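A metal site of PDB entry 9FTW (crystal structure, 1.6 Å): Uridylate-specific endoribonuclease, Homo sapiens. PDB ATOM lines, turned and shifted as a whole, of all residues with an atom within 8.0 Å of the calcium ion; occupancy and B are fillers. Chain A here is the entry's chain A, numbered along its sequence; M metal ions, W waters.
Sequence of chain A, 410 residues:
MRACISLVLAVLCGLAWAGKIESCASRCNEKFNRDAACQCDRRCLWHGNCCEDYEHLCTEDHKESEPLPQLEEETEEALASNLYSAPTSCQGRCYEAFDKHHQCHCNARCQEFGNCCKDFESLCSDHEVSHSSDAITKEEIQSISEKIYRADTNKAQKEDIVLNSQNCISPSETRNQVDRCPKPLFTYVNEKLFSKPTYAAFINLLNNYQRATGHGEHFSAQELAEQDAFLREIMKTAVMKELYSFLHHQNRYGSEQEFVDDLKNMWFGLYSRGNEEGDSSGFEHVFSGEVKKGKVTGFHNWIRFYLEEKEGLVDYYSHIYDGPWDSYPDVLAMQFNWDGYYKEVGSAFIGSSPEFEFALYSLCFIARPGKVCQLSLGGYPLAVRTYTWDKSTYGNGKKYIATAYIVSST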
ATOM      1  N   ASN A 208     -23.049   3.037   4.411  1.00  0.00           N
ATOM      2  CA  ASN A 208     -24.366   3.152   5.056  1.00  0.00           C
ATOM      3  C   ASN A 208     -25.442   3.880   4.216  1.00  0.00           C
ATOM      4  O   ASN A 208     -26.574   4.002   4.697  1.00  0.00           O
ATOM      5  CB  ASN A 208     -24.245   3.924   6.373  1.00  0.00           C
ATOM      6  CG  ASN A 208     -23.412   3.249   7.422  1.00  0.00           C
ATOM      7  OD1 ASN A 208     -22.828   2.173   7.173  1.00  0.00           O
ATOM      8  ND2 ASN A 208     -23.355   3.832   8.623  1.00  0.00           N
ATOM      9  N   TYR A 209     -25.116   4.366   3.011  1.00  0.00           N
ATOM     10  CA  TYR A 209     -26.025   5.249   2.278  1.00  0.00           C
ATOM     11  C   TYR A 209     -26.420   4.753   0.881  1.00  0.00           C
ATOM     12  O   TYR A 209     -25.805   3.832   0.347  1.00  0.00           O
ATOM     13  CB  TYR A 209     -25.288   6.626   2.146  1.00  0.00           C
ATOM     14  CG  TYR A 209     -24.991   7.249   3.500  1.00  0.00           C
ATOM     15  CD1 TYR A 209     -25.960   7.962   4.183  1.00  0.00           C
ATOM     16  CD2 TYR A 209     -23.760   7.051   4.123  1.00  0.00           C
ATOM     17  CE1 TYR A 209     -25.713   8.487   5.435  1.00  0.00           C
ATOM     18  CE2 TYR A 209     -23.518   7.513   5.400  1.00  0.00           C
ATOM     19  CZ  TYR A 209     -24.481   8.295   6.038  1.00  0.00           C
ATOM     20  OH  TYR A 209     -24.292   8.772   7.311  1.00  0.00           O
ATOM     21  N   GLN A 210     -27.439   5.402   0.308  1.00  0.00           N
ATOM     22  CA  GLN A 210     -27.908   5.202  -1.075  1.00  0.00           C
ATOM     23  C   GLN A 210     -27.622   6.575  -1.726  1.00  0.00           C
ATOM     24  O   GLN A 210     -28.210   7.578  -1.332  1.00  0.00           O
ATOM     25  CB  GLN A 210     -29.411   4.857  -1.105  1.00  0.00           C
ATOM     26  CG  GLN A 210     -29.739   3.623  -0.274  1.00  0.00           C
ATOM     27  CD  GLN A 210     -31.189   3.595   0.165  1.00  0.00           C
ATOM     28  OE1 GLN A 210     -31.556   4.148   1.211  1.00  0.00           O
ATOM     29  NE2 GLN A 210     -32.056   2.960  -0.643  1.00  0.00           N
ATOM     30  N   ARG A 211     -26.665   6.628  -2.640  1.00  0.00           N
ATOM     31  CA  ARG A 211     -26.253   7.904  -3.244  1.00  0.00           C
ATOM     32  C   ARG A 211     -27.366   8.636  -3.972  1.00  0.00           C
ATOM     33  O   ARG A 211     -27.377   9.872  -3.972  1.00  0.00           O
ATOM     34  CB  ARG A 211     -25.031   7.744  -4.161  1.00  0.00           C
ATOM     35  CG  ARG A 211     -25.291   6.908  -5.402  1.00  0.00           C
ATOM     36  CD  ARG A 211     -24.107   6.840  -6.337  1.00  0.00           C
ATOM     37  NE  ARG A 211     -24.515   6.185  -7.587  1.00  0.00           N
ATOM     38  CZ  ARG A 211     -23.858   6.251  -8.735  1.00  0.00           C
ATOM     39  NH1 ARG A 211     -22.732   6.949  -8.836  1.00  0.00           N
ATOM     40  NH2 ARG A 211     -24.317   5.597  -9.807  1.00  0.00           N
ATOM     41  N   ALA A 212     -28.265   7.905  -4.660  1.00  0.00           N
ATOM     42  CA  ALA A 212     -29.335   8.587  -5.402  1.00  0.00           C
ATOM     43  C   ALA A 212     -30.318   9.149  -4.421  1.00  0.00           C
ATOM     44  O   ALA A 212     -30.846   8.419  -3.573  1.00  0.00           O
ATOM     45  CB  ALA A 212     -30.040   7.611  -6.319  1.00  0.00           C
ATOM     46  N   THR A 213     -30.567  10.451  -4.512  1.00  0.00           N
ATOM     47  CA  THR A 213     -31.622  11.075  -3.691  1.00  0.00           C
ATOM     48  C   THR A 213     -32.974  10.466  -4.158  1.00  0.00           C
ATOM     49  O   THR A 213     -33.071   9.909  -5.252  1.00  0.00           O
ATOM     50  CB  THR A 213     -31.633  12.600  -3.902  1.00  0.00           C
ATOM     51  OG1 THR A 213     -31.842  12.861  -5.298  1.00  0.00           O
ATOM     52  CG2 THR A 213     -30.363  13.286  -3.401  1.00  0.00           C
ATOM     53  N   GLY A 214     -33.974  10.533  -3.304  1.00  0.00           N
ATOM     54  CA  GLY A 214     -35.273   9.939  -3.584  1.00  0.00           C
ATOM     55  C   GLY A 214     -35.450   8.561  -2.964  1.00  0.00           C
ATOM     56  O   GLY A 214     -36.473   7.916  -3.198  1.00  0.00           O
ATOM     57  N   HIS A 215     -34.458   8.090  -2.176  1.00  0.00           N
ATOM     58  CA  HIS A 215     -34.515   6.792  -1.527  1.00  0.00           C
ATOM     59  C   HIS A 215     -34.231   7.036  -0.064  1.00  0.00           C
ATOM     60  O   HIS A 215     -33.104   7.343   0.295  1.00  0.00           O
ATOM     61  CB  HIS A 215     -33.474   5.850  -2.144  1.00  0.00           C
ATOM     62  CG  HIS A 215     -33.635   5.692  -3.625  1.00  0.00           C
ATOM     63  ND1 HIS A 215     -34.412   4.681  -4.170  1.00  0.00           N
ATOM     64  CD2 HIS A 215     -33.097   6.419  -4.640  1.00  0.00           C
ATOM     65  CE1 HIS A 215     -34.294   4.800  -5.481  1.00  0.00           C
ATOM     66  NE2 HIS A 215     -33.562   5.864  -5.807  1.00  0.00           N
ATOM     67  N   GLY A 216     -35.256   6.918   0.774  1.00  0.00           N
ATOM     68  CA  GLY A 216     -35.097   7.157   2.207  1.00  0.00           C
ATOM     69  C   GLY A 216     -34.034   6.276   2.853  1.00  0.00           C
ATOM     70  O   GLY A 216     -33.909   5.099   2.502  1.00  0.00           O
ATOM     71  N   GLU A 217     -33.268   6.855   3.800  1.00  0.00           N
ATOM     72  CA  GLU A 217     -32.232   6.113   4.537  1.00  0.00           C
ATOM     73  C   GLU A 217     -32.823   5.572   5.839  1.00  0.00           C
ATOM     74  O   GLU A 217     -33.596   6.257   6.514  1.00  0.00           O
ATOM     75  CB  GLU A 217     -31.016   7.004   4.889  1.00  0.00           C
ATOM     76  CG  GLU A 217     -30.309   7.670   3.727  1.00  0.00           C
ATOM     77  CD  GLU A 217     -29.594   6.776   2.724  1.00  0.00           C
ATOM     78  OE1 GLU A 217     -29.593   5.536   2.913  1.00  0.00           O
ATOM     79  OE2 GLU A 217     -29.014   7.313   1.758  1.00  0.00           O
ATOM     80  N   PHE A 219     -31.193   3.577   9.100  1.00  0.00           N
ATOM     81  CA  PHE A 219     -29.980   2.994   9.670  1.00  0.00           C
ATOM     82  C   PHE A 219     -30.289   1.904  10.659  1.00  0.00           C
ATOM     83  O   PHE A 219     -31.276   1.992  11.392  1.00  0.00           O
ATOM     84  CB  PHE A 219     -29.108   4.052  10.339  1.00  0.00           C
ATOM     85  CG  PHE A 219     -28.719   5.159   9.382  1.00  0.00           C
ATOM     86  CD1 PHE A 219     -28.153   4.865   8.154  1.00  0.00           C
ATOM     87  CD2 PHE A 219     -28.984   6.485   9.694  1.00  0.00           C
ATOM     88  CE1 PHE A 219     -27.845   5.887   7.264  1.00  0.00           C
ATOM     89  CE2 PHE A 219     -28.646   7.494   8.807  1.00  0.00           C
ATOM     90  CZ  PHE A 219     -28.087   7.190   7.608  1.00  0.00           C
ATOM     91  N   LEU A 270     -31.047  13.200   9.443  1.00  0.00           N
ATOM     92  CA  LEU A 270     -31.569  13.044   8.092  1.00  0.00           C
ATOM     93  C   LEU A 270     -32.535  14.160   7.695  1.00  0.00           C
ATOM     94  O   LEU A 270     -33.310  14.668   8.506  1.00  0.00           O
ATOM     95  CB  LEU A 270     -32.242  11.666   7.957  1.00  0.00           C
ATOM     96  CG  LEU A 270     -31.359  10.429   8.112  1.00  0.00           C
ATOM     97  CD1 LEU A 270     -32.228   9.187   8.182  1.00  0.00           C
ATOM     98  CD2 LEU A 270     -30.351  10.309   6.964  1.00  0.00           C
ATOM     99  N   TYR A 271     -32.487  14.528   6.411  1.00  0.00           N
ATOM    100  CA  TYR A 271     -33.441  15.485   5.834  1.00  0.00           C
ATOM    101  C   TYR A 271     -33.743  15.047   4.380  1.00  0.00           C
ATOM    102  O   TYR A 271     -33.217  14.013   3.936  1.00  0.00           O
ATOM    103  CB  TYR A 271     -32.959  16.924   6.004  1.00  0.00           C
ATOM    104  CG  TYR A 271     -31.574  17.173   5.462  1.00  0.00           C
ATOM    105  CD1 TYR A 271     -31.342  17.281   4.109  1.00  0.00           C
ATOM    106  CD2 TYR A 271     -30.497  17.362   6.328  1.00  0.00           C
ATOM    107  CE1 TYR A 271     -30.089  17.598   3.604  1.00  0.00           C
ATOM    108  CE2 TYR A 271     -29.248  17.704   5.841  1.00  0.00           C
ATOM    109  CZ  TYR A 271     -29.031  17.784   4.481  1.00  0.00           C
ATOM    110  OH  TYR A 271     -27.781  18.065   3.987  1.00  0.00           O
ATOM    111  N   ARG A 273     -33.697  15.741   0.353  1.00  0.00           N
ATOM    112  CA  ARG A 273     -33.307  16.445  -0.873  1.00  0.00           C
ATOM    113  C   ARG A 273     -34.217  16.049  -2.070  1.00  0.00           C
ATOM    114  O   ARG A 273     -34.525  16.902  -2.913  1.00  0.00           O
ATOM    115  CB  ARG A 273     -31.847  16.140  -1.246  1.00  0.00           C
ATOM    116  CG  ARG A 273     -30.814  17.001  -0.553  1.00  0.00           C
ATOM    117  CD  ARG A 273     -29.430  16.832  -1.174  1.00  0.00           C
ATOM    118  NE  ARG A 273     -28.616  18.022  -0.890  1.00  0.00           N
ATOM    119  CZ  ARG A 273     -27.846  18.216   0.176  1.00  0.00           C
ATOM    120  NH1 ARG A 273     -27.680  17.234   1.071  1.00  0.00           N
ATOM    121  NH2 ARG A 273     -27.186  19.353   0.333  1.00  0.00           N
ATOM    122  N   GLY A 278     -36.076  11.828   4.512  1.00  0.00           N
ATOM    123  CA  GLY A 278     -34.835  11.345   5.097  1.00  0.00           C
ATOM    124  C   GLY A 278     -33.876  10.646   4.141  1.00  0.00           C
ATOM    125  O   GLY A 278     -33.228   9.671   4.544  1.00  0.00           O
ATOM    126  N   ASP A 279     -33.751  11.135   2.897  1.00  0.00           N
ATOM    127  CA  ASP A 279     -32.809  10.520   1.947  1.00  0.00           C
ATOM    128  C   ASP A 279     -31.392  11.137   2.002  1.00  0.00           C
ATOM    129  O   ASP A 279     -30.488  10.646   1.303  1.00  0.00           O
ATOM    130  CB  ASP A 279     -33.351  10.653   0.507  1.00  0.00           C
ATOM    131  CG  ASP A 279     -33.469  12.078  -0.001  1.00  0.00           C
ATOM    132  OD1 ASP A 279     -33.222  13.010   0.774  1.00  0.00           O
ATOM    133  OD2 ASP A 279     -33.845  12.246  -1.177  1.00  0.00           O
ATOM    134  N   SER A 280     -31.178  12.197   2.810  1.00  0.00           N
ATOM    135  CA  SER A 280     -29.899  12.907   2.773  1.00  0.00           C
ATOM    136  C   SER A 280     -29.460  13.441   4.149  1.00  0.00           C
ATOM    137  O   SER A 280     -30.175  13.335   5.149  1.00  0.00           O
ATOM    138  CB  SER A 280     -30.003  14.031   1.743  1.00  0.00           C
ATOM    139  OG  SER A 280     -28.742  14.577   1.369  1.00  0.00           O
ATOM    140  N   SER A 281     -28.217  13.893   4.211  1.00  0.00           N
ATOM    141  CA  SER A 281     -27.650  14.475   5.439  1.00  0.00           C
ATOM    142  C   SER A 281     -26.398  15.233   5.069  1.00  0.00           C
ATOM    143  O   SER A 281     -25.835  15.004   3.983  1.00  0.00           O
ATOM    144  CB  SER A 281     -27.319  13.379   6.449  1.00  0.00           C
ATOM    145  OG  SER A 281     -26.442  12.398   5.900  1.00  0.00           O
ATOM    146  N   GLU A 284     -23.579  12.535   4.570  1.00  0.00           N
ATOM    147  CA  GLU A 284     -23.696  11.837   3.280  1.00  0.00           C
ATOM    148  C   GLU A 284     -23.282  12.758   2.129  1.00  0.00           C
ATOM    149  O   GLU A 284     -22.475  12.365   1.290  1.00  0.00           O
ATOM    150  CB  GLU A 284     -25.124  11.346   3.026  1.00  0.00           C
ATOM    151  CG  GLU A 284     -25.203  10.594   1.706  1.00  0.00           C
ATOM    152  CD  GLU A 284     -26.529   9.999   1.347  1.00  0.00           C
ATOM    153  OE1 GLU A 284     -27.531  10.307   2.034  1.00  0.00           O
ATOM    154  OE2 GLU A 284     -26.575   9.261   0.334  1.00  0.00           O
ATOM    155  N   HIS A 285     -23.800  13.990   2.115  1.00  0.00           N
ATOM    156  CA  HIS A 285     -23.500  14.903   1.000  1.00  0.00           C
ATOM    157  C   HIS A 285     -22.005  15.169   0.839  1.00  0.00           C
ATOM    158  O   HIS A 285     -21.447  15.007  -0.251  1.00  0.00           O
ATOM    159  CB  HIS A 285     -24.290  16.211   1.196  1.00  0.00           C
ATOM    160  CG  HIS A 285     -24.208  17.121   0.029  1.00  0.00           C
ATOM    161  ND1 HIS A 285     -24.931  16.880  -1.122  1.00  0.00           N
ATOM    162  CD2 HIS A 285     -23.511  18.275  -0.130  1.00  0.00           C
ATOM    163  CE1 HIS A 285     -24.664  17.890  -1.943  1.00  0.00           C
ATOM    164  NE2 HIS A 285     -23.825  18.755  -1.383  1.00  0.00           N
ATOM    165  N   SER A 288     -19.848  11.101   1.529  1.00  0.00           N
ATOM    166  CA  SER A 288     -20.199   9.944   0.714  1.00  0.00           C
ATOM    167  C   SER A 288     -20.438  10.318  -0.725  1.00  0.00           C
ATOM    168  O   SER A 288     -20.066   9.559  -1.616  1.00  0.00           O
ATOM    169  CB  SER A 288     -21.407   9.225   1.296  1.00  0.00           C
ATOM    170  OG  SER A 288     -21.727   8.075   0.514  1.00  0.00           O
ATOM    171  N   GLY A 289     -21.092  11.462  -0.977  1.00  0.00           N
ATOM    172  CA  GLY A 289     -21.421  11.904  -2.327  1.00  0.00           C
ATOM    173  C   GLY A 289     -22.814  11.452  -2.692  1.00  0.00           C
ATOM    174  O   GLY A 289     -23.306  10.430  -2.189  1.00  0.00           O
ATOM    175  N   GLU A 290     -23.509  12.233  -3.521  1.00  0.00           N
ATOM    176  CA  GLU A 290     -24.873  11.891  -3.930  1.00  0.00           C
ATOM    177  C   GLU A 290     -25.056  12.044  -5.444  1.00  0.00           C
ATOM    178  O   GLU A 290     -24.157  12.551  -6.133  1.00  0.00           O
ATOM    179  CB  GLU A 290     -25.877  12.802  -3.202  1.00  0.00           C
ATOM    180  CG  GLU A 290     -25.824  12.712  -1.701  1.00  0.00           C
ATOM    181  CD  GLU A 290     -26.831  13.637  -1.068  1.00  0.00           C
ATOM    182  OE1 GLU A 290     -26.586  14.861  -1.009  1.00  0.00           O
ATOM    183  OE2 GLU A 290     -27.895  13.133  -0.630  1.00  0.00           O
ATOM    184  N   VAL A 291     -26.182  11.545  -5.976  1.00  0.00           N
ATOM    185  CA  VAL A 291     -26.544  11.703  -7.392  1.00  0.00           C
ATOM    186  C   VAL A 291     -27.949  12.310  -7.388  1.00  0.00           C
ATOM    187  O   VAL A 291     -28.879  11.717  -6.809  1.00  0.00           O
ATOM    188  CB  VAL A 291     -26.453  10.382  -8.194  1.00  0.00           C
ATOM    189  CG1 VAL A 291     -27.072  10.553  -9.583  1.00  0.00           C
ATOM    190  CG2 VAL A 291     -25.006   9.906  -8.300  1.00  0.00           C
HETATM  191 CA    CA M   1     -28.978   9.138   0.277  1.00  0.00          CA
HETATM  192  O   HOH W   1     -28.755  10.748  -1.428  1.00  0.00           O
HETATM  193  O   HOH W   2     -31.038   8.438  -0.641  1.00  0.00           O
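Water W1 bridges OE2 of Glu 290 and O of Arg 211.
Of the 24 residues printed, 4 come within 4 Å of the calcium ion.
The calcium ion is bound by the side-chain carboxylate (OE2) of Glu 217 (2.4 Å), water W1 (2.4 Å), water W2 (2.4 Å), the backbone carbonyl oxygen (O) of Asp 279 (2.4 Å), the backbone carbonyl oxygen (O) of Gln 210 (2.4 Å), the side-chain carboxylate (OE2) of Glu 284 (2.4 Å) and the side-chain carboxylate (OE1) of Glu 284 (2.6 Å).
The backbone NH (N) of Glu 217 lies within hydrogen-bond range of the backbone carbonyl oxygen (O) of Gly 278, 2.9 Å away.
The backbone NH of Gly 214 lies within hydrogen-bond range of the side-chain carboxylate of Asp 279 (2.7 Å).
N of Asp 279 sits at hydrogen-bond distance from O of Tyr 271 (3.1 Å).
The side-chain carboxylate (OD1) of Asp 279 sits at hydrogen-bond distance from the backbone NH (N) of Arg 273 (2.8 Å).
The backbone carbonyl oxygen (O) of Gly 216 sits close to the side-chain amide oxygen (OE1) of Gln 210, at 2.8 Å.
N of Glu 284 sits at hydrogen-bond distance from OG of Ser 281 (3.2 Å).
O of Glu 284 sits at hydrogen-bond distance from N of Gly 289 (2.8 Å).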
